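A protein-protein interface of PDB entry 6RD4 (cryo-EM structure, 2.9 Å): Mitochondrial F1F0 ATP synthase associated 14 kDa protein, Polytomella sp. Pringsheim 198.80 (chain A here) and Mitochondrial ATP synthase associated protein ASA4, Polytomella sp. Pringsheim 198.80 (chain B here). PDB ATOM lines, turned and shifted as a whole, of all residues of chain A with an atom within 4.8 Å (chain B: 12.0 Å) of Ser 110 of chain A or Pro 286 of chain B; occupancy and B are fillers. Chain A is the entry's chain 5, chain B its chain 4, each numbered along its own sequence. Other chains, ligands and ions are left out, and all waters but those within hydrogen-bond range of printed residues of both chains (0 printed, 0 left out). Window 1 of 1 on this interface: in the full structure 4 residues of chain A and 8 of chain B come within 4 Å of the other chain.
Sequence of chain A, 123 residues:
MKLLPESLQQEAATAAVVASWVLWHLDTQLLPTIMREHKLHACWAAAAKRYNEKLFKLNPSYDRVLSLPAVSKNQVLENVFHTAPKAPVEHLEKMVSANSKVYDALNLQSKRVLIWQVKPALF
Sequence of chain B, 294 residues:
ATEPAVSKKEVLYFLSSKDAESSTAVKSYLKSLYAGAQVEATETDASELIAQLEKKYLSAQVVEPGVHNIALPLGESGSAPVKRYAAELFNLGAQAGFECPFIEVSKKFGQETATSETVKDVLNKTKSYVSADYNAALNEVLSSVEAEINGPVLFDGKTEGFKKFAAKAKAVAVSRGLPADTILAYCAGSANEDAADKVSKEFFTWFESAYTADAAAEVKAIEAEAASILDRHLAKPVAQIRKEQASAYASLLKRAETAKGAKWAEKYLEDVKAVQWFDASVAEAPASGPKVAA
The side-chain hydroxyl (OG) of Ser 110 of chain A lies within hydrogen-bond range of the backbone NH (N) of Arg 112 of chain A.
The side-chain hydroxyl of Ser 288 of chain B is in hydrogen-bond range of the side-chain amino group of Lys 291 of chain B, 3.5 Å away.
The backbone carbonyl oxygen (O) of Gly 289 of chain B is in hydrogen-bond range of the side-chain amino group (NZ) of Lys 291 of chain B (3.2 Å).
The side-chain hydroxyl (OG) of Ser 110 of chain A is in hydrogen-bond range of the backbone carbonyl oxygen (O) of Asp 104 of chain A.
Printed residues of chain B that touch a printed residue of chain A: Phe 278, Val 282, Ala 283, Pro 286, Ser 288 and Gly 289.
Hydrophobic or aromatic side chains of chain B within 4 Å of the printed part of chain A: Phe 278, Val 282, Ala 283 and Pro 286.
Along chain B the printed residues that touch a printed residue of chain A span positions 278 to 289.
Hydrophobic or aromatic side chains of chain A within 4 Å of the printed part of chain B: Trp 116.
No residue of chain B comes within 4 Å of Asp 104 of chain A.
No residue of chain B comes within 4 Å of Asn 107 of chain A.
No residue of chain B comes within 4 Å of Gln 109 of chain A.
Ser 110 of chain A touches just one residue of chain B: Pro 286 (3.2 Å).
Of chain B, only Ala 283 comes within 4 Å of Lys 111 of chain A.
No residue of chain B comes within 4 Å of Arg 112 of chain A.
Printed residues of chain A within 4 Å of Phe 278 of chain B: Trp 116 (3.6 Å).
Of the printed residues of chain A, Ala 283 of chain B touches Lys 111.
Pro 286 of chain B touches just these residues of chain A: Ser 110 (3.2 Å) and Trp 116 (3.0 Å).
Printed residues of chain A within 4 Å of Ser 288 of chain B: Trp 116.
The nearest residue of chain B that does not touch Ser 110 of chain A is Val 282 of chain B (5.2 Å).
The nearest printed residue of chain A that does not touch Ser 288 of chain B is Leu 108 of chain A (6.5 Å).
The backbone carbonyl oxygen (O) of Pro 286 of chain B is in hydrogen-bond range of the indole nitrogen (NE1) of Trp 116 of chain A (3.0 Å).
Among the printed residues, pairs that only touch across the chains: Ser 110 of chain A with Pro 286 of chain B (3.2 Å), Lys 111 of chain A with Ala 283 of chain B (3.3 Å), Trp 116 of chain A with Phe 278 of chain B (3.6 Å), Trp 116 of chain A with Val 282 of chain B (3.6 Å), Trp 116 of chain A with Ser 288 of chain B (3.8 Å) and Trp 116 of chain A with Gly 289 of chain B (3.5 Å).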
ATOM      1  N   TYR A 103      25.434 -13.006 -18.647  1.00  0.00           N
ATOM      2  CA  TYR A 103      24.328 -13.894 -18.331  1.00  0.00           C
ATOM      3  C   TYR A 103      24.500 -15.220 -19.025  1.00  0.00           C
ATOM      4  O   TYR A 103      24.260 -16.260 -18.418  1.00  0.00           O
ATOM      5  CB  TYR A 103      22.983 -13.300 -18.734  1.00  0.00           C
ATOM      6  CG  TYR A 103      21.820 -14.237 -18.482  1.00  0.00           C
ATOM      7  CD1 TYR A 103      21.290 -14.375 -17.233  1.00  0.00           C
ATOM      8  CD2 TYR A 103      21.265 -14.991 -19.501  1.00  0.00           C
ATOM      9  CE1 TYR A 103      20.256 -15.206 -17.002  1.00  0.00           C
ATOM     10  CE2 TYR A 103      20.248 -15.850 -19.257  1.00  0.00           C
ATOM     11  CZ  TYR A 103      19.748 -15.946 -18.010  1.00  0.00           C
ATOM     12  OH  TYR A 103      18.717 -16.794 -17.754  1.00  0.00           O
ATOM     13  N   ASP A 104      24.872 -15.196 -20.302  1.00  0.00           N
ATOM     14  CA  ASP A 104      24.932 -16.417 -21.091  1.00  0.00           C
ATOM     15  C   ASP A 104      25.954 -17.374 -20.530  1.00  0.00           C
ATOM     16  O   ASP A 104      25.643 -18.523 -20.236  1.00  0.00           O
ATOM     17  CB  ASP A 104      25.269 -16.097 -22.533  1.00  0.00           C
ATOM     18  CG  ASP A 104      24.100 -15.580 -23.289  1.00  0.00           C
ATOM     19  OD1 ASP A 104      23.027 -15.463 -22.680  1.00  0.00           O
ATOM     20  OD2 ASP A 104      24.246 -15.280 -24.488  1.00  0.00           O
ATOM     21  N   ASN A 107      25.461 -18.206 -15.770  1.00  0.00           N
ATOM     22  CA  ASN A 107      24.264 -18.049 -14.950  1.00  0.00           C
ATOM     23  C   ASN A 107      23.805 -19.275 -14.193  1.00  0.00           C
ATOM     24  O   ASN A 107      23.420 -19.128 -13.031  1.00  0.00           O
ATOM     25  CB  ASN A 107      23.082 -17.582 -15.766  1.00  0.00           C
ATOM     26  CG  ASN A 107      21.984 -17.076 -14.896  1.00  0.00           C
ATOM     27  OD1 ASN A 107      22.071 -15.999 -14.350  1.00  0.00           O
ATOM     28  ND2 ASN A 107      20.922 -17.840 -14.785  1.00  0.00           N
ATOM     29  N   LEU A 108      23.840 -20.453 -14.827  1.00  0.00           N
ATOM     30  CA  LEU A 108      23.312 -21.797 -14.504  1.00  0.00           C
ATOM     31  C   LEU A 108      21.902 -22.017 -15.012  1.00  0.00           C
ATOM     32  O   LEU A 108      21.420 -23.127 -14.910  1.00  0.00           O
ATOM     33  CB  LEU A 108      23.303 -22.183 -13.017  1.00  0.00           C
ATOM     34  CG  LEU A 108      24.688 -22.210 -12.400  1.00  0.00           C
ATOM     35  CD1 LEU A 108      24.619 -22.459 -10.905  1.00  0.00           C
ATOM     36  CD2 LEU A 108      25.507 -23.262 -13.097  1.00  0.00           C
ATOM     37  N   GLN A 109      21.237 -21.023 -15.565  1.00  0.00           N
ATOM     38  CA  GLN A 109      19.986 -21.267 -16.254  1.00  0.00           C
ATOM     39  C   GLN A 109      20.058 -20.904 -17.717  1.00  0.00           C
ATOM     40  O   GLN A 109      19.054 -21.028 -18.416  1.00  0.00           O
ATOM     41  CB  GLN A 109      18.826 -20.498 -15.621  1.00  0.00           C
ATOM     42  CG  GLN A 109      18.089 -21.223 -14.526  1.00  0.00           C
ATOM     43  CD  GLN A 109      18.790 -21.145 -13.210  1.00  0.00           C
ATOM     44  OE1 GLN A 109      19.150 -22.161 -12.627  1.00  0.00           O
ATOM     45  NE2 GLN A 109      18.989 -19.933 -12.724  1.00  0.00           N
ATOM     46  N   SER A 110      21.203 -20.458 -18.196  1.00  0.00           N
ATOM     47  CA  SER A 110      21.335 -20.078 -19.582  1.00  0.00           C
ATOM     48  C   SER A 110      21.416 -21.304 -20.466  1.00  0.00           C
ATOM     49  O   SER A 110      21.780 -22.377 -20.034  1.00  0.00           O
ATOM     50  CB  SER A 110      22.575 -19.235 -19.762  1.00  0.00           C
ATOM     51  OG  SER A 110      22.816 -19.006 -21.127  1.00  0.00           O
ATOM     52  N   LYS A 111      21.094 -21.134 -21.731  1.00  0.00           N
ATOM     53  CA  LYS A 111      21.223 -22.271 -22.623  1.00  0.00           C
ATOM     54  C   LYS A 111      22.659 -22.515 -23.035  1.00  0.00           C
ATOM     55  O   LYS A 111      22.953 -23.577 -23.580  1.00  0.00           O
ATOM     56  CB  LYS A 111      20.360 -22.083 -23.862  1.00  0.00           C
ATOM     57  CG  LYS A 111      18.891 -21.926 -23.569  1.00  0.00           C
ATOM     58  CD  LYS A 111      18.371 -23.059 -22.718  1.00  0.00           C
ATOM     59  CE  LYS A 111      16.954 -22.802 -22.246  1.00  0.00           C
ATOM     60  NZ  LYS A 111      16.510 -23.807 -21.249  1.00  0.00           N
ATOM     61  N   ARG A 112      23.564 -21.561 -22.803  1.00  0.00           N
ATOM     62  CA  ARG A 112      24.975 -21.742 -23.122  1.00  0.00           C
ATOM     63  C   ARG A 112      25.825 -21.405 -21.916  1.00  0.00           C
ATOM     64  O   ARG A 112      26.589 -20.458 -21.986  1.00  0.00           O
ATOM     65  CB  ARG A 112      25.355 -20.858 -24.288  1.00  0.00           C
ATOM     66  CG  ARG A 112      24.694 -21.233 -25.573  1.00  0.00           C
ATOM     67  CD  ARG A 112      24.898 -20.215 -26.656  1.00  0.00           C
ATOM     68  NE  ARG A 112      24.072 -19.037 -26.467  1.00  0.00           N
ATOM     69  CZ  ARG A 112      24.545 -17.801 -26.432  1.00  0.00           C
ATOM     70  NH1 ARG A 112      23.716 -16.787 -26.264  1.00  0.00           N
ATOM     71  NH2 ARG A 112      25.841 -17.576 -26.586  1.00  0.00           N
ATOM     72  N   VAL A 113      25.848 -22.253 -20.920  1.00  0.00           N
ATOM     73  CA  VAL A 113      26.608 -21.951 -19.720  1.00  0.00           C
ATOM     74  C   VAL A 113      28.000 -22.491 -19.944  1.00  0.00           C
ATOM     75  O   VAL A 113      28.181 -23.468 -20.672  1.00  0.00           O
ATOM     76  CB  VAL A 113      25.997 -22.589 -18.465  1.00  0.00           C
ATOM     77  CG1 VAL A 113      26.393 -21.830 -17.244  1.00  0.00           C
ATOM     78  CG2 VAL A 113      24.589 -22.670 -18.555  1.00  0.00           C
ATOM     79  N   TRP A 116      29.742 -26.512 -17.752  1.00  0.00           N
ATOM     80  CA  TRP A 116      30.052 -27.864 -18.163  1.00  0.00           C
ATOM     81  C   TRP A 116      31.230 -27.896 -19.098  1.00  0.00           C
ATOM     82  O   TRP A 116      31.697 -28.972 -19.454  1.00  0.00           O
ATOM     83  CB  TRP A 116      28.839 -28.505 -18.825  1.00  0.00           C
ATOM     84  CG  TRP A 116      27.612 -28.250 -18.072  1.00  0.00           C
ATOM     85  CD1 TRP A 116      26.601 -27.444 -18.434  1.00  0.00           C
ATOM     86  CD2 TRP A 116      27.268 -28.783 -16.799  1.00  0.00           C
ATOM     87  NE1 TRP A 116      25.638 -27.436 -17.476  1.00  0.00           N
ATOM     88  CE2 TRP A 116      26.030 -28.251 -16.454  1.00  0.00           C
ATOM     89  CE3 TRP A 116      27.891 -29.660 -15.917  1.00  0.00           C
ATOM     90  CZ2 TRP A 116      25.396 -28.570 -15.278  1.00  0.00           C
ATOM     91  CZ3 TRP A 116      27.266 -29.966 -14.750  1.00  0.00           C
ATOM     92  CH2 TRP A 116      26.033 -29.427 -14.436  1.00  0.00           C
ATOM     93  N   TRP B 277      26.899 -32.004 -30.162  1.00  0.00           N
ATOM     94  CA  TRP B 277      25.953 -32.700 -29.307  1.00  0.00           C
ATOM     95  C   TRP B 277      26.047 -32.194 -27.876  1.00  0.00           C
ATOM     96  O   TRP B 277      25.033 -32.106 -27.183  1.00  0.00           O
ATOM     97  CB  TRP B 277      26.186 -34.208 -29.364  1.00  0.00           C
ATOM     98  CG  TRP B 277      25.329 -34.971 -28.415  1.00  0.00           C
ATOM     99  CD1 TRP B 277      24.101 -35.474 -28.659  1.00  0.00           C
ATOM    100  CD2 TRP B 277      25.639 -35.311 -27.061  1.00  0.00           C
ATOM    101  NE1 TRP B 277      23.615 -36.102 -27.543  1.00  0.00           N
ATOM    102  CE2 TRP B 277      24.546 -36.012 -26.547  1.00  0.00           C
ATOM    103  CE3 TRP B 277      26.735 -35.075 -26.234  1.00  0.00           C
ATOM    104  CZ2 TRP B 277      24.517 -36.482 -25.249  1.00  0.00           C
ATOM    105  CZ3 TRP B 277      26.700 -35.538 -24.952  1.00  0.00           C
ATOM    106  CH2 TRP B 277      25.607 -36.233 -24.471  1.00  0.00           C
ATOM    107  N   PHE B 278      27.256 -31.891 -27.406  1.00  0.00           N
ATOM    108  CA  PHE B 278      27.434 -31.430 -26.034  1.00  0.00           C
ATOM    109  C   PHE B 278      26.806 -30.067 -25.833  1.00  0.00           C
ATOM    110  O   PHE B 278      26.224 -29.794 -24.782  1.00  0.00           O
ATOM    111  CB  PHE B 278      28.918 -31.377 -25.686  1.00  0.00           C
ATOM    112  CG  PHE B 278      29.199 -31.307 -24.219  1.00  0.00           C
ATOM    113  CD1 PHE B 278      29.259 -30.091 -23.560  1.00  0.00           C
ATOM    114  CD2 PHE B 278      29.431 -32.448 -23.504  1.00  0.00           C
ATOM    115  CE1 PHE B 278      29.519 -30.029 -22.230  1.00  0.00           C
ATOM    116  CE2 PHE B 278      29.692 -32.381 -22.171  1.00  0.00           C
ATOM    117  CZ  PHE B 278      29.739 -31.169 -21.537  1.00  0.00           C
ATOM    118  N   ASP B 279      26.918 -29.197 -26.827  1.00  0.00           N
ATOM    119  CA  ASP B 279      26.299 -27.891 -26.725  1.00  0.00           C
ATOM    120  C   ASP B 279      24.793 -27.982 -26.842  1.00  0.00           C
ATOM    121  O   ASP B 279      24.080 -27.149 -26.278  1.00  0.00           O
ATOM    122  CB  ASP B 279      26.856 -26.973 -27.799  1.00  0.00           C
ATOM    123  CG  ASP B 279      28.320 -26.698 -27.619  1.00  0.00           C
ATOM    124  OD1 ASP B 279      28.795 -26.754 -26.470  1.00  0.00           O
ATOM    125  OD2 ASP B 279      28.995 -26.410 -28.624  1.00  0.00           O
ATOM    126  N   ALA B 280      24.290 -28.980 -27.562  1.00  0.00           N
ATOM    127  CA  ALA B 280      22.853 -29.132 -27.724  1.00  0.00           C
ATOM    128  C   ALA B 280      22.235 -29.860 -26.547  1.00  0.00           C
ATOM    129  O   ALA B 280      21.113 -29.549 -26.151  1.00  0.00           O
ATOM    130  CB  ALA B 280      22.546 -29.876 -29.016  1.00  0.00           C
ATOM    131  N   SER B 281      22.943 -30.826 -25.976  1.00  0.00           N
ATOM    132  CA  SER B 281      22.432 -31.525 -24.809  1.00  0.00           C
ATOM    133  C   SER B 281      22.432 -30.663 -23.565  1.00  0.00           C
ATOM    134  O   SER B 281      21.666 -30.936 -22.644  1.00  0.00           O
ATOM    135  CB  SER B 281      23.250 -32.776 -24.544  1.00  0.00           C
ATOM    136  OG  SER B 281      22.802 -33.417 -23.378  1.00  0.00           O
ATOM    137  N   VAL B 282      23.286 -29.649 -23.506  1.00  0.00           N
ATOM    138  CA  VAL B 282      23.284 -28.733 -22.375  1.00  0.00           C
ATOM    139  C   VAL B 282      22.163 -27.724 -22.523  1.00  0.00           C
ATOM    140  O   VAL B 282      21.508 -27.367 -21.539  1.00  0.00           O
ATOM    141  CB  VAL B 282      24.670 -28.084 -22.257  1.00  0.00           C
ATOM    142  CG1 VAL B 282      24.642 -26.819 -21.448  1.00  0.00           C
ATOM    143  CG2 VAL B 282      25.612 -29.050 -21.626  1.00  0.00           C
ATOM    144  N   ALA B 283      21.872 -27.312 -23.755  1.00  0.00           N
ATOM    145  CA  ALA B 283      20.774 -26.402 -24.031  1.00  0.00           C
ATOM    146  C   ALA B 283      19.414 -26.997 -23.710  1.00  0.00           C
ATOM    147  O   ALA B 283      18.467 -26.247 -23.481  1.00  0.00           O
ATOM    148  CB  ALA B 283      20.812 -25.986 -25.493  1.00  0.00           C
ATOM    149  N   GLU B 284      19.290 -28.319 -23.679  1.00  0.00           N
ATOM    150  CA  GLU B 284      18.018 -28.924 -23.325  1.00  0.00           C
ATOM    151  C   GLU B 284      17.761 -28.906 -21.827  1.00  0.00           C
ATOM    152  O   GLU B 284      16.613 -28.744 -21.411  1.00  0.00           O
ATOM    153  CB  GLU B 284      17.957 -30.351 -23.849  1.00  0.00           C
ATOM    154  CG  GLU B 284      18.003 -30.447 -25.358  1.00  0.00           C
ATOM    155  CD  GLU B 284      18.296 -31.853 -25.827  1.00  0.00           C
ATOM    156  OE1 GLU B 284      18.427 -32.749 -24.967  1.00  0.00           O
ATOM    157  OE2 GLU B 284      18.403 -32.066 -27.051  1.00  0.00           O
ATOM    158  N   ALA B 285      18.792 -29.065 -20.998  1.00  0.00           N
ATOM    159  CA  ALA B 285      18.639 -28.938 -19.549  1.00  0.00           C
ATOM    160  C   ALA B 285      19.945 -28.471 -18.945  1.00  0.00           C
ATOM    161  O   ALA B 285      20.835 -29.273 -18.655  1.00  0.00           O
ATOM    162  CB  ALA B 285      18.187 -30.245 -18.904  1.00  0.00           C
ATOM    163  N   PRO B 286      20.089 -27.168 -18.717  1.00  0.00           N
ATOM    164  CA  PRO B 286      21.379 -26.641 -18.265  1.00  0.00           C
ATOM    165  C   PRO B 286      21.678 -26.858 -16.799  1.00  0.00           C
ATOM    166  O   PRO B 286      22.852 -26.850 -16.425  1.00  0.00           O
ATOM    167  CB  PRO B 286      21.258 -25.156 -18.580  1.00  0.00           C
ATOM    168  CG  PRO B 286      20.139 -25.064 -19.535  1.00  0.00           C
ATOM    169  CD  PRO B 286      19.198 -26.091 -19.158  1.00  0.00           C
ATOM    170  N   ALA B 287      20.682 -26.992 -15.940  1.00  0.00           N
ATOM    171  CA  ALA B 287      20.999 -27.316 -14.562  1.00  0.00           C
ATOM    172  C   ALA B 287      21.345 -28.783 -14.384  1.00  0.00           C
ATOM    173  O   ALA B 287      21.912 -29.153 -13.353  1.00  0.00           O
ATOM    174  CB  ALA B 287      19.837 -26.945 -13.652  1.00  0.00           C
ATOM    175  N   SER B 288      21.015 -29.620 -15.362  1.00  0.00           N
ATOM    176  CA  SER B 288      21.345 -31.034 -15.356  1.00  0.00           C
ATOM    177  C   SER B 288      22.709 -31.301 -15.960  1.00  0.00           C
ATOM    178  O   SER B 288      23.504 -32.051 -15.391  1.00  0.00           O
ATOM    179  CB  SER B 288      20.283 -31.815 -16.127  1.00  0.00           C
ATOM    180  OG  SER B 288      20.705 -33.137 -16.385  1.00  0.00           O
ATOM    181  N   GLY B 289      23.005 -30.681 -17.090  1.00  0.00           N
ATOM    182  CA  GLY B 289      24.231 -30.931 -17.794  1.00  0.00           C
ATOM    183  C   GLY B 289      23.980 -31.695 -19.068  1.00  0.00           C
ATOM    184  O   GLY B 289      22.882 -31.668 -19.622  1.00  0.00           O
ATOM    185  N   PRO B 290      24.999 -32.379 -19.571  1.00  0.00           N
ATOM    186  CA  PRO B 290      24.787 -33.273 -20.706  1.00  0.00           C
ATOM    187  C   PRO B 290      24.059 -34.535 -20.283  1.00  0.00           C
ATOM    188  O   PRO B 290      24.132 -34.970 -19.134  1.00  0.00           O
ATOM    189  CB  PRO B 290      26.208 -33.582 -21.175  1.00  0.00           C
ATOM    190  CG  PRO B 290      27.016 -33.413 -19.981  1.00  0.00           C
ATOM    191  CD  PRO B 290      26.420 -32.285 -19.222  1.00  0.00           C
ATOM    192  N   LYS B 291      23.342 -35.122 -21.234  1.00  0.00           N
ATOM    193  CA  LYS B 291      22.574 -36.331 -20.982  1.00  0.00           C
ATOM    194  C   LYS B 291      23.448 -37.550 -21.207  1.00  0.00           C
ATOM    195  O   LYS B 291      23.930 -37.767 -22.317  1.00  0.00           O
ATOM    196  CB  LYS B 291      21.364 -36.387 -21.908  1.00  0.00           C
ATOM    197  CG  LYS B 291      20.433 -35.236 -21.727  1.00  0.00           C
ATOM    198  CD  LYS B 291      19.757 -35.316 -20.378  1.00  0.00           C
ATOM    199  CE  LYS B 291      19.016 -34.033 -20.069  1.00  0.00           C
ATOM    200  NZ  LYS B 291      19.995 -32.958 -19.783  1.00  0.00           N
ATOM    201  N   VAL B 292      23.640 -38.354 -20.181  1.00  0.00           N
ATOM    202  CA  VAL B 292      24.316 -39.618 -20.358  1.00  0.00           C
ATOM    203  C   VAL B 292      23.273 -40.721 -20.377  1.00  0.00           C
ATOM    204  O   VAL B 292      22.131 -40.549 -19.943  1.00  0.00           O
ATOM    205  CB  VAL B 292      25.374 -39.880 -19.270  1.00  0.00           C
ATOM    206  CG1 VAL B 292      26.283 -38.706 -19.150  1.00  0.00           C
ATOM    207  CG2 VAL B 292      24.705 -40.166 -17.958  1.00  0.00           C
